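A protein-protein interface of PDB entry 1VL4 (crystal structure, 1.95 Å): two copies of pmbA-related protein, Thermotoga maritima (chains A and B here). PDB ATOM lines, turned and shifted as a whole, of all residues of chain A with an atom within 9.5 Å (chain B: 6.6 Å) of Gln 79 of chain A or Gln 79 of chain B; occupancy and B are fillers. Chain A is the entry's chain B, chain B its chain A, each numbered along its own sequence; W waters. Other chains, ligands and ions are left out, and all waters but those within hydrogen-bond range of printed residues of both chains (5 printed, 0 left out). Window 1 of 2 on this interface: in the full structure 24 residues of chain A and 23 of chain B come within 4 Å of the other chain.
Leu 38 of chain A touches none of the printed residues of chain B. Printed residues of chain B within 4 Å of Asp 57 of chain A: Arg 77. Printed residues of chain B within 4 Å of Phe 61 of chain A: Gln 79 (2.8 Å). Ile 65 of chain A touches none of the printed residues of chain B. Of chain B, only Gly 59, Lys 60, Phe 61 and Gln 79 come within 4 Å of Gln 79 of chain A. Of the printed residues of chain A, Gly 59 of chain B touches Arg 77, Thr 78 and Gln 79. Lys 60 of chain B touches just one residue of chain A: Gln 79 (3.2 Å). Printed residues of chain A within 4 Å of Arg 77 of chain B: Asp 57 (3.0 Å), Ala 58 (3.3 Å) and Gly 59 (2.9 Å). Of chain A, only Gly 59, Lys 60, Phe 61 and Gln 79 come within 4 Å of Gln 79 of chain B. Val 80 of chain B touches none of the printed residues of chain A. The nearest printed residue of chain B that does not touch Asp 57 of chain A is Thr 78 of chain B (5.7 Å).
Gly 59 of chain A touches Arg 77 of chain B, and with the chains exchanged Arg 77 of chain A touches Gly 59 of chain B. Gly 59 of chain A touches Gln 79 of chain B, and with the chains exchanged Gln 79 of chain A touches Gly 59 of chain B. Phe 61 of chain A touches Gln 79 of chain B, and with the chains exchanged Gln 79 of chain A touches Phe 61 of chain B. Gln 79 of chain A touches its own counterpart, Gln 79 of chain B. Of the 13 pairs that touch across the chains among the printed residues, 11 have their exchanged pair printed and touching as well.
Among the printed residues, pairs that only touch across the chains: Gln 79 of chain A with Lys 60 of chain B, Lys 60 of chain A with Gln 79 of chain B, Ala 58 of chain A with Arg 77 of chain B, Thr 78 of chain A with Gly 59 of chain B and Gly 59 of chain A with Thr 78 of chain B.
Water W1 lies within hydrogen-bond range of ND2 of Asn 62 of chain A and O of Gly 59 of chain B. Water W4 bridges the backbone carbonyl oxygen (O) of Gln 79 of chain A (2.6 Å) and the backbone carbonyl oxygen (O) of Gln 79 of chain B (2.8 Å). Water W5 lies within hydrogen-bond range of OG1 of Thr 78 of chain B, N of Gln 79 of chain B and O of Gly 59 of chain A. Water W2 lies within hydrogen-bond range of the backbone NH of Gln 79 of chain A (3.0 Å), the backbone carbonyl oxygen of Gly 59 of chain B (3.1 Å) and the side-chain hydroxyl of Thr 78 of chain A (3.3 Å). Water W3 lies within hydrogen-bond range of O of Gly 59 of chain A (3.1 Å) and OD1 of Asn 62 of chain B (3.3 Å).
Along chain A the printed residues that touch a printed residue of chain B span positions 57 to 79. Of the 11 printed residues of chain B, 6 touch a printed residue of chain A.
The backbone NH (N) of Val 63 of chain B is in hydrogen-bond range of the backbone carbonyl oxygen (O) of Thr 78 of chain B (2.7 Å). The backbone carbonyl oxygen of Thr 40 of chain A lies within hydrogen-bond range of the backbone NH of Lys 60 of chain A. N of Glu 42 of chain A is in hydrogen-bond range of O of Ala 58 of chain A, at 3.0 Å. The side-chain amino group (NZ) of Lys 60 of chain A lies within salt-bridge range of the side-chain carboxylate (OE1) of Glu 42 of chain A, at 3.7 Å. O of Thr 78 of chain A sits at hydrogen-bond distance from ND2 of Asn 62 of chain A (3.2 Å). The side-chain hydroxyl (OG1) of Thr 78 of chain A is in hydrogen-bond range of the backbone carbonyl oxygen (O) of Val 80 of chain A, 3.2 Å away.
The backbone carbonyl oxygen (O) of Arg 77 of chain A sits at hydrogen-bond distance from the backbone NH (N) of Gly 59 of chain B (2.8 Å). O of Gly 59 of chain B is in hydrogen-bond range of N of Gln 79 of chain A (3.3 Å). N of Phe 61 of chain B lies within hydrogen-bond range of OE1 of Gln 79 of chain A, at 2.9 Å. N of Arg 77 of chain B is in hydrogen-bond range of O of Asp 57 of chain A (3.0 Å). The backbone carbonyl oxygen of Arg 77 of chain B lies within hydrogen-bond range of the backbone NH of Gly 59 of chain A (2.9 Å). The backbone carbonyl oxygen (O) of Gly 59 of chain A sits at hydrogen-bond distance from the backbone NH (N) of Gln 79 of chain B, 3.4 Å away. OE1 of Gln 79 of chain B lies within hydrogen-bond range of N of Phe 61 of chain A, at 2.8 Å. The side-chain amide nitrogen (NE2) of Gln 79 of chain A is in hydrogen-bond range of the side-chain amide oxygen (OE1) of Gln 79 of chain B (3.4 Å).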
ATOM      1  N   PHE A  18      19.356  -1.234  -5.202  1.00  0.00           N
ATOM      2  CA  PHE A  18      19.855  -0.419  -6.321  1.00  0.00           C
ATOM      3  C   PHE A  18      20.446  -1.301  -7.471  1.00  0.00           C
ATOM      4  O   PHE A  18      20.064  -1.164  -8.657  1.00  0.00           O
ATOM      5  CB  PHE A  18      20.904   0.546  -5.772  1.00  0.00           C
ATOM      6  CG  PHE A  18      21.253   1.683  -6.684  1.00  0.00           C
ATOM      7  CD1 PHE A  18      20.423   2.798  -6.777  1.00  0.00           C
ATOM      8  CD2 PHE A  18      22.436   1.656  -7.423  1.00  0.00           C
ATOM      9  CE1 PHE A  18      20.770   3.887  -7.600  1.00  0.00           C
ATOM     10  CE2 PHE A  18      22.783   2.737  -8.248  1.00  0.00           C
ATOM     11  CZ  PHE A  18      21.962   3.846  -8.330  1.00  0.00           C
ATOM     12  N   SER A  36      30.330   0.343  -9.821  1.00  0.00           N
ATOM     13  CA  SER A  36      31.485   0.453  -8.984  1.00  0.00           C
ATOM     14  C   SER A  36      31.111   1.368  -7.852  1.00  0.00           C
ATOM     15  O   SER A  36      30.622   2.508  -8.068  1.00  0.00           O
ATOM     16  CB  SER A  36      32.699   1.033  -9.719  1.00  0.00           C
ATOM     17  OG  SER A  36      33.084   0.256 -10.823  1.00  0.00           O
ATOM     18  N   LEU A  38      32.464   3.020  -4.152  1.00  0.00           N
ATOM     19  CA  LEU A  38      33.633   3.440  -3.329  1.00  0.00           C
ATOM     20  C   LEU A  38      33.135   4.177  -2.135  1.00  0.00           C
ATOM     21  O   LEU A  38      32.398   5.150  -2.271  1.00  0.00           O
ATOM     22  CB  LEU A  38      34.561   4.335  -4.106  1.00  0.00           C
ATOM     23  CG  LEU A  38      35.824   4.740  -3.323  1.00  0.00           C
ATOM     24  CD1 LEU A  38      36.656   3.506  -2.881  1.00  0.00           C
ATOM     25  CD2 LEU A  38      36.669   5.740  -4.145  1.00  0.00           C
ATOM     26  N   GLU A  39      33.467   3.693  -0.947  1.00  0.00           N
ATOM     27  CA  GLU A  39      33.067   4.353   0.291  1.00  0.00           C
ATOM     28  C   GLU A  39      34.303   4.466   1.190  1.00  0.00           C
ATOM     29  O   GLU A  39      35.010   3.471   1.373  1.00  0.00           O
ATOM     30  CB  GLU A  39      32.018   3.496   0.968  1.00  0.00           C
ATOM     31  CG  GLU A  39      31.525   3.944   2.319  1.00  0.00           C
ATOM     32  CD  GLU A  39      30.379   3.054   2.780  1.00  0.00           C
ATOM     33  OE1 GLU A  39      30.643   1.865   3.088  1.00  0.00           O
ATOM     34  OE2 GLU A  39      29.214   3.533   2.779  1.00  0.00           O
ATOM     35  N   THR A  40      34.582   5.675   1.681  1.00  0.00           N
ATOM     36  CA  THR A  40      35.815   5.993   2.429  1.00  0.00           C
ATOM     37  C   THR A  40      35.513   6.778   3.685  1.00  0.00           C
ATOM     38  O   THR A  40      34.523   7.580   3.749  1.00  0.00           O
ATOM     39  CB  THR A  40      36.797   6.809   1.592  1.00  0.00           C
ATOM     40  OG1 THR A  40      36.335   8.149   1.462  1.00  0.00           O
ATOM     41  CG2 THR A  40      36.932   6.223   0.224  1.00  0.00           C
ATOM     42  N   ARG A  41      36.325   6.554   4.709  1.00  0.00           N
ATOM     43  CA  ARG A  41      36.297   7.417   5.872  1.00  0.00           C
ATOM     44  C   ARG A  41      37.766   7.753   6.155  1.00  0.00           C
ATOM     45  O   ARG A  41      38.643   6.882   6.089  1.00  0.00           O
ATOM     46  CB  ARG A  41      35.681   6.683   7.076  1.00  0.00           C
ATOM     47  CG  ARG A  41      34.216   7.045   7.471  1.00  0.00           C
ATOM     48  CD  ARG A  41      34.034   8.492   8.009  1.00  0.00           C
ATOM     49  NE  ARG A  41      35.166   8.898   8.846  1.00  0.00           N
ATOM     50  CZ  ARG A  41      35.140   9.071  10.168  1.00  0.00           C
ATOM     51  NH1 ARG A  41      36.267   9.401  10.792  1.00  0.00           N
ATOM     52  NH2 ARG A  41      34.019   8.931  10.880  1.00  0.00           N
ATOM     53  N   GLU A  42      38.039   8.998   6.479  1.00  0.00           N
ATOM     54  CA  GLU A  42      39.403   9.450   6.718  1.00  0.00           C
ATOM     55  C   GLU A  42      39.399  10.449   7.837  1.00  0.00           C
ATOM     56  O   GLU A  42      38.416  11.163   8.066  1.00  0.00           O
ATOM     57  CB  GLU A  42      39.941  10.088   5.457  1.00  0.00           C
ATOM     58  CG  GLU A  42      39.127  11.263   5.029  1.00  0.00           C
ATOM     59  CD  GLU A  42      39.518  11.871   3.689  1.00  0.00           C
ATOM     60  OE1 GLU A  42      39.194  11.280   2.633  1.00  0.00           O
ATOM     61  OE2 GLU A  42      40.084  12.994   3.709  1.00  0.00           O
ATOM     62  N   ASP A  57      37.773  15.339   9.146  1.00  0.00           N
ATOM     63  CA  ASP A  57      37.053  14.121   9.524  1.00  0.00           C
ATOM     64  C   ASP A  57      35.898  14.028   8.534  1.00  0.00           C
ATOM     65  O   ASP A  57      34.979  14.865   8.523  1.00  0.00           O
ATOM     66  CB  ASP A  57      36.649  14.217  11.002  1.00  0.00           C
ATOM     67  CG  ASP A  57      35.984  12.968  11.538  1.00  0.00           C
ATOM     68  OD1 ASP A  57      35.983  11.919  10.862  1.00  0.00           O
ATOM     69  OD2 ASP A  57      35.477  13.027  12.678  1.00  0.00           O
ATOM     70  N   ALA A  58      35.968  13.034   7.660  1.00  0.00           N
ATOM     71  CA  ALA A  58      35.113  13.044   6.507  1.00  0.00           C
ATOM     72  C   ALA A  58      34.799  11.641   6.014  1.00  0.00           C
ATOM     73  O   ALA A  58      35.695  10.749   5.987  1.00  0.00           O
ATOM     74  CB  ALA A  58      35.838  13.834   5.402  1.00  0.00           C
ATOM     75  N   GLY A  59      33.536  11.446   5.632  1.00  0.00           N
ATOM     76  CA  GLY A  59      33.100  10.223   4.957  1.00  0.00           C
ATOM     77  C   GLY A  59      32.673  10.564   3.547  1.00  0.00           C
ATOM     78  O   GLY A  59      32.042  11.593   3.334  1.00  0.00           O
ATOM     79  N   LYS A  60      33.035   9.710   2.587  1.00  0.00           N
ATOM     80  CA  LYS A  60      32.714   9.948   1.195  1.00  0.00           C
ATOM     81  C   LYS A  60      32.120   8.689   0.570  1.00  0.00           C
ATOM     82  O   LYS A  60      32.401   7.584   1.009  1.00  0.00           O
ATOM     83  CB  LYS A  60      33.972  10.381   0.453  1.00  0.00           C
ATOM     84  CG  LYS A  60      34.533  11.710   0.973  1.00  0.00           C
ATOM     85  CD  LYS A  60      35.868  12.059   0.331  1.00  0.00           C
ATOM     86  CE  LYS A  60      36.381  13.446   0.847  1.00  0.00           C
ATOM     87  NZ  LYS A  60      37.744  13.731   0.318  1.00  0.00           N
ATOM     88  N   PHE A  61      31.359   8.868  -0.508  1.00  0.00           N
ATOM     89  CA  PHE A  61      30.703   7.766  -1.138  1.00  0.00           C
ATOM     90  C   PHE A  61      30.565   8.113  -2.632  1.00  0.00           C
ATOM     91  O   PHE A  61      30.095   9.187  -2.943  1.00  0.00           O
ATOM     92  CB  PHE A  61      29.317   7.610  -0.447  1.00  0.00           C
ATOM     93  CG  PHE A  61      28.427   6.575  -1.086  1.00  0.00           C
ATOM     94  CD1 PHE A  61      28.724   5.229  -0.975  1.00  0.00           C
ATOM     95  CD2 PHE A  61      27.284   6.955  -1.781  1.00  0.00           C
ATOM     96  CE1 PHE A  61      27.899   4.262  -1.578  1.00  0.00           C
ATOM     97  CE2 PHE A  61      26.458   6.021  -2.375  1.00  0.00           C
ATOM     98  CZ  PHE A  61      26.749   4.671  -2.268  1.00  0.00           C
ATOM     99  N   ASN A  62      30.974   7.227  -3.535  1.00  0.00           N
ATOM    100  CA  ASN A  62      30.634   7.414  -4.961  1.00  0.00           C
ATOM    101  C   ASN A  62      30.211   6.098  -5.602  1.00  0.00           C
ATOM    102  O   ASN A  62      30.843   5.051  -5.355  1.00  0.00           O
ATOM    103  CB  ASN A  62      31.819   8.011  -5.743  1.00  0.00           C
ATOM    104  CG  ASN A  62      31.421   9.343  -6.536  1.00  0.00           C
ATOM    105  OD1 ASN A  62      31.981  10.427  -6.284  1.00  0.00           O
ATOM    106  ND2 ASN A  62      30.442   9.245  -7.457  1.00  0.00           N
ATOM    107  N   VAL A  63      29.169   6.162  -6.433  1.00  0.00           N
ATOM    108  CA  VAL A  63      28.805   5.042  -7.318  1.00  0.00           C
ATOM    109  C   VAL A  63      28.943   5.482  -8.764  1.00  0.00           C
ATOM    110  O   VAL A  63      28.462   6.567  -9.163  1.00  0.00           O
ATOM    111  CB  VAL A  63      27.375   4.543  -7.034  1.00  0.00           C
ATOM    112  CG1 VAL A  63      26.998   3.365  -7.912  1.00  0.00           C
ATOM    113  CG2 VAL A  63      27.258   4.145  -5.583  1.00  0.00           C
ATOM    114  N   GLU A  64      29.589   4.634  -9.546  1.00  0.00           N
ATOM    115  CA  GLU A  64      29.642   4.757 -10.990  1.00  0.00           C
ATOM    116  C   GLU A  64      28.820   3.664 -11.674  1.00  0.00           C
ATOM    117  O   GLU A  64      29.017   2.455 -11.440  1.00  0.00           O
ATOM    118  CB  GLU A  64      31.093   4.714 -11.466  1.00  0.00           C
ATOM    119  CG  GLU A  64      31.204   4.852 -12.970  1.00  0.00           C
ATOM    120  CD  GLU A  64      32.574   4.517 -13.538  1.00  0.00           C
ATOM    121  OE1 GLU A  64      32.914   3.316 -13.681  1.00  0.00           O
ATOM    122  OE2 GLU A  64      33.285   5.470 -13.907  1.00  0.00           O
ATOM    123  N   ILE A  65      27.914   4.101 -12.519  1.00  0.00           N
ATOM    124  CA  ILE A  65      27.109   3.228 -13.319  1.00  0.00           C
ATOM    125  C   ILE A  65      27.620   3.279 -14.749  1.00  0.00           C
ATOM    126  O   ILE A  65      27.666   4.351 -15.364  1.00  0.00           O
ATOM    127  CB  ILE A  65      25.648   3.652 -13.303  1.00  0.00           C
ATOM    128  CG1 ILE A  65      25.102   3.613 -11.864  1.00  0.00           C
ATOM    129  CG2 ILE A  65      24.773   2.718 -14.177  1.00  0.00           C
ATOM    130  CD1 ILE A  65      24.976   4.897 -11.169  1.00  0.00           C
ATOM    131  N   PHE A  76      27.562   7.226 -15.773  1.00  0.00           N
ATOM    132  CA  PHE A  76      27.005   8.250 -14.895  1.00  0.00           C
ATOM    133  C   PHE A  76      27.504   7.958 -13.483  1.00  0.00           C
ATOM    134  O   PHE A  76      27.552   6.823 -13.070  1.00  0.00           O
ATOM    135  CB  PHE A  76      25.500   8.324 -14.940  1.00  0.00           C
ATOM    136  CG  PHE A  76      24.920   9.352 -14.014  1.00  0.00           C
ATOM    137  CD1 PHE A  76      25.174  10.707 -14.215  1.00  0.00           C
ATOM    138  CD2 PHE A  76      24.102   8.982 -12.975  1.00  0.00           C
ATOM    139  CE1 PHE A  76      24.663  11.686 -13.358  1.00  0.00           C
ATOM    140  CE2 PHE A  76      23.537   9.975 -12.084  1.00  0.00           C
ATOM    141  CZ  PHE A  76      23.832  11.316 -12.280  1.00  0.00           C
ATOM    142  N   ARG A  77      27.951   9.009 -12.793  1.00  0.00           N
ATOM    143  CA  ARG A  77      28.416   8.895 -11.423  1.00  0.00           C
ATOM    144  C   ARG A  77      27.494   9.636 -10.502  1.00  0.00           C
ATOM    145  O   ARG A  77      27.117  10.801 -10.760  1.00  0.00           O
ATOM    146  CB  ARG A  77      29.821   9.464 -11.307  1.00  0.00           C
ATOM    147  CG  ARG A  77      30.919   8.467 -11.713  1.00  0.00           C
ATOM    148  CD  ARG A  77      32.396   8.940 -11.461  1.00  0.00           C
ATOM    149  NE  ARG A  77      33.272   8.411 -12.518  1.00  0.00           N
ATOM    150  CZ  ARG A  77      33.169   8.738 -13.816  1.00  0.00           C
ATOM    151  NH1 ARG A  77      32.229   9.601 -14.230  1.00  0.00           N
ATOM    152  NH2 ARG A  77      34.003   8.193 -14.709  1.00  0.00           N
ATOM    153  N   THR A  78      27.186   9.016  -9.365  1.00  0.00           N
ATOM    154  CA  THR A  78      26.297   9.635  -8.364  1.00  0.00           C
ATOM    155  C   THR A  78      26.817   9.360  -6.923  1.00  0.00           C
ATOM    156  O   THR A  78      27.434   8.324  -6.674  1.00  0.00           O
ATOM    157  CB  THR A  78      24.875   9.139  -8.574  1.00  0.00           C
ATOM    158  OG1 THR A  78      23.976   9.847  -7.701  1.00  0.00           O
ATOM    159  CG2 THR A  78      24.744   7.603  -8.349  1.00  0.00           C
ATOM    160  N   GLN A  79      26.586  10.296  -6.002  1.00  0.00           N
ATOM    161  CA  GLN A  79      26.999  10.179  -4.561  1.00  0.00           C
ATOM    162  C   GLN A  79      25.739   9.965  -3.738  1.00  0.00           C
ATOM    163  O   GLN A  79      25.733  10.278  -2.544  1.00  0.00           O
ATOM    164  CB  GLN A  79      27.768  11.448  -4.085  1.00  0.00           C
ATOM    165  CG  GLN A  79      29.156  11.525  -4.744  1.00  0.00           C
ATOM    166  CD  GLN A  79      30.066  12.663  -4.336  1.00  0.00           C
ATOM    167  OE1 GLN A  79      29.646  13.718  -3.837  1.00  0.00           O
ATOM    168  NE2 GLN A  79      31.355  12.464  -4.599  1.00  0.00           N
ATOM    169  N   VAL A  80      24.671   9.489  -4.414  1.00  0.00           N
ATOM    170  CA  VAL A  80      23.365   9.183  -3.812  1.00  0.00           C
ATOM    171  C   VAL A  80      22.679   7.938  -4.448  1.00  0.00           C
ATOM    172  O   VAL A  80      22.400   7.910  -5.650  1.00  0.00           O
ATOM    173  CB  VAL A  80      22.349  10.387  -3.911  1.00  0.00           C
ATOM    174  CG1 VAL A  80      21.033  10.032  -3.256  1.00  0.00           C
ATOM    175  CG2 VAL A  80      22.904  11.697  -3.287  1.00  0.00           C
ATOM    176  N   LEU A  81      22.382   6.925  -3.635  1.00  0.00           N
ATOM    177  CA  LEU A  81      21.701   5.709  -4.103  1.00  0.00           C
ATOM    178  C   LEU A  81      20.218   5.891  -4.179  1.00  0.00           C
ATOM    179  O   LEU A  81      19.468   5.326  -3.378  1.00  0.00           O
ATOM    180  CB  LEU A  81      21.940   4.523  -3.173  1.00  0.00           C
ATOM    181  CG  LEU A  81      23.260   3.770  -3.067  1.00  0.00           C
ATOM    182  CD1 LEU A  81      22.998   2.575  -2.165  1.00  0.00           C
ATOM    183  CD2 LEU A  81      23.860   3.279  -4.389  1.00  0.00           C
ATOM    184  N   GLU A  82      19.748   6.660  -5.145  1.00  0.00           N
ATOM    185  CA  GLU A  82      18.313   6.728  -5.373  1.00  0.00           C
ATOM    186  C   GLU A  82      18.106   6.749  -6.872  1.00  0.00           C
ATOM    187  O   GLU A  82      19.059   6.970  -7.607  1.00  0.00           O
ATOM    188  CB  GLU A  82      17.719   7.964  -4.685  1.00  0.00           C
ATOM    189  N   CYS A  87      19.368   6.990 -13.258  1.00  0.00           N
ATOM    190  CA  CYS A  87      20.802   6.771 -13.425  1.00  0.00           C
ATOM    191  C   CYS A  87      21.108   5.924 -14.652  1.00  0.00           C
ATOM    192  O   CYS A  87      22.062   6.226 -15.380  1.00  0.00           O
ATOM    193  CB  CYS A  87      21.379   6.049 -12.202  1.00  0.00           C
ATOM    194  SG  CYS A  87      21.318   7.055 -10.683  1.00  0.00           S
ATOM    195  N   THR B  40      25.878  19.400  -6.514  1.00  0.00           N
ATOM    196  CA  THR B  40      26.386  19.737  -7.825  1.00  0.00           C
ATOM    197  C   THR B  40      26.079  18.657  -8.865  1.00  0.00           C
ATOM    198  O   THR B  40      25.999  17.454  -8.567  1.00  0.00           O
ATOM    199  CB  THR B  40      27.901  19.959  -7.812  1.00  0.00           C
ATOM    200  OG1 THR B  40      28.576  18.720  -7.933  1.00  0.00           O
ATOM    201  CG2 THR B  40      28.330  20.665  -6.606  1.00  0.00           C
ATOM    202  N   GLY B  59      26.971  13.602 -10.486  1.00  0.00           N
ATOM    203  CA  GLY B  59      26.313  14.333  -9.430  1.00  0.00           C
ATOM    204  C   GLY B  59      26.986  14.085  -8.071  1.00  0.00           C
ATOM    205  O   GLY B  59      27.410  12.953  -7.774  1.00  0.00           O
ATOM    206  N   LYS B  60      27.122  15.168  -7.290  1.00  0.00           N
ATOM    207  CA  LYS B  60      27.886  15.162  -6.036  1.00  0.00           C
ATOM    208  C   LYS B  60      27.073  15.846  -4.945  1.00  0.00           C
ATOM    209  O   LYS B  60      26.253  16.680  -5.230  1.00  0.00           O
ATOM    210  CB  LYS B  60      29.206  15.950  -6.206  1.00  0.00           C
ATOM    211  CG  LYS B  60      30.173  15.368  -7.226  1.00  0.00           C
ATOM    212  CD  LYS B  60      31.426  16.259  -7.341  1.00  0.00           C
ATOM    213  N   PHE B  61      27.347  15.495  -3.695  1.00  0.00           N
ATOM    214  CA  PHE B  61      26.592  15.975  -2.578  1.00  0.00           C
ATOM    215  C   PHE B  61      27.506  15.941  -1.354  1.00  0.00           C
ATOM    216  O   PHE B  61      28.092  14.905  -1.066  1.00  0.00           O
ATOM    217  CB  PHE B  61      25.426  14.997  -2.416  1.00  0.00           C
ATOM    218  CG  PHE B  61      24.641  15.222  -1.219  1.00  0.00           C
ATOM    219  CD1 PHE B  61      23.917  16.390  -1.092  1.00  0.00           C
ATOM    220  CD2 PHE B  61      24.661  14.297  -0.163  1.00  0.00           C
ATOM    221  CE1 PHE B  61      23.185  16.638   0.068  1.00  0.00           C
ATOM    222  CE2 PHE B  61      23.932  14.509   0.974  1.00  0.00           C
ATOM    223  CZ  PHE B  61      23.185  15.679   1.109  1.00  0.00           C
ATOM    224  N   ASN B  62      27.671  17.061  -0.672  1.00  0.00           N
ATOM    225  CA  ASN B  62      28.476  17.147   0.549  1.00  0.00           C
ATOM    226  C   ASN B  62      27.675  17.860   1.655  1.00  0.00           C
ATOM    227  O   ASN B  62      27.090  18.905   1.399  1.00  0.00           O
ATOM    228  CB  ASN B  62      29.755  17.969   0.268  1.00  0.00           C
ATOM    229  CG  ASN B  62      30.871  17.135  -0.315  1.00  0.00           C
ATOM    230  OD1 ASN B  62      31.431  16.238   0.355  1.00  0.00           O
ATOM    231  ND2 ASN B  62      31.201  17.405  -1.578  1.00  0.00           N
ATOM    232  N   VAL B  63      27.647  17.303   2.860  1.00  0.00           N
ATOM    233  CA  VAL B  63      27.066  18.006   4.007  1.00  0.00           C
ATOM    234  C   VAL B  63      28.148  18.181   5.088  1.00  0.00           C
ATOM    235  O   VAL B  63      28.803  17.217   5.435  1.00  0.00           O
ATOM    236  CB  VAL B  63      25.882  17.242   4.555  1.00  0.00           C
ATOM    237  CG1 VAL B  63      25.313  17.966   5.702  1.00  0.00           C
ATOM    238  CG2 VAL B  63      24.851  17.132   3.489  1.00  0.00           C
ATOM    239  N   ARG B  77      32.204  15.916   8.041  1.00  0.00           N
ATOM    240  CA  ARG B  77      31.705  16.017   6.666  1.00  0.00           C
ATOM    241  C   ARG B  77      31.223  14.644   6.235  1.00  0.00           C
ATOM    242  O   ARG B  77      31.851  13.604   6.520  1.00  0.00           O
ATOM    243  CB  ARG B  77      32.766  16.572   5.705  1.00  0.00           C
ATOM    244  CG  ARG B  77      33.266  17.983   6.115  1.00  0.00           C
ATOM    245  CD  ARG B  77      33.905  18.762   4.960  1.00  0.00           C
ATOM    246  N   THR B  78      30.080  14.635   5.566  1.00  0.00           N
ATOM    247  CA  THR B  78      29.423  13.376   5.139  1.00  0.00           C
ATOM    248  C   THR B  78      28.847  13.636   3.731  1.00  0.00           C
ATOM    249  O   THR B  78      28.569  14.781   3.380  1.00  0.00           O
ATOM    250  CB  THR B  78      28.386  12.898   6.151  1.00  0.00           C
ATOM    251  OG1 THR B  78      27.936  11.592   5.781  1.00  0.00           O
ATOM    252  CG2 THR B  78      27.188  13.841   6.262  1.00  0.00           C
ATOM    253  N   GLN B  79      28.853  12.600   2.895  1.00  0.00           N
ATOM    254  CA  GLN B  79      28.212  12.619   1.586  1.00  0.00           C
ATOM    255  C   GLN B  79      26.928  11.759   1.687  1.00  0.00           C
ATOM    256  O   GLN B  79      26.386  11.401   0.684  1.00  0.00           O
ATOM    257  CB  GLN B  79      29.155  12.100   0.481  1.00  0.00           C
ATOM    258  CG  GLN B  79      30.095  13.150   0.003  1.00  0.00           C
ATOM    259  CD  GLN B  79      31.177  12.669  -0.913  1.00  0.00           C
ATOM    260  OE1 GLN B  79      31.223  11.495  -1.311  1.00  0.00           O
ATOM    261  NE2 GLN B  79      32.088  13.580  -1.261  1.00  0.00           N
ATOM    262  N   VAL B  80      26.458  11.455   2.893  1.00  0.00           N
ATOM    263  CA  VAL B  80      25.237  10.663   3.099  1.00  0.00           C
ATOM    264  C   VAL B  80      24.343  11.306   4.159  1.00  0.00           C
ATOM    265  O   VAL B  80      24.785  11.570   5.280  1.00  0.00           O
ATOM    266  CB  VAL B  80      25.546   9.207   3.563  1.00  0.00           C
ATOM    267  CG1 VAL B  80      24.258   8.423   3.759  1.00  0.00           C
ATOM    268  CG2 VAL B  80      26.463   8.460   2.572  1.00  0.00           C
ATOM    269  N   LEU B  81      23.067  11.521   3.831  1.00  0.00           N
ATOM    270  CA  LEU B  81      22.134  12.139   4.770  1.00  0.00           C
ATOM    271  C   LEU B  81      21.581  11.107   5.663  1.00  0.00           C
ATOM    272  O   LEU B  81      20.380  10.841   5.630  1.00  0.00           O
ATOM    273  CB  LEU B  81      20.950  12.838   4.060  1.00  0.00           C
ATOM    274  CG  LEU B  81      21.041  14.293   3.632  1.00  0.00           C
ATOM    275  CD1 LEU B  81      19.656  14.916   3.526  1.00  0.00           C
ATOM    276  CD2 LEU B  81      21.883  15.098   4.605  1.00  0.00           C
HETATM  277  O   HOH W   1      30.284  11.660  -8.392  1.00  0.00           O
HETATM  278  O   HOH W   2      24.711  12.674  -6.188  1.00  0.00           O
HETATM  279  O   HOH W   3      32.853  14.506   2.710  1.00  0.00           O
HETATM  280  O   HOH W   4      24.216  10.006  -0.450  1.00  0.00           O
HETATM  281  O   HOH W   5      29.628   9.895   3.982  1.00  0.00           O
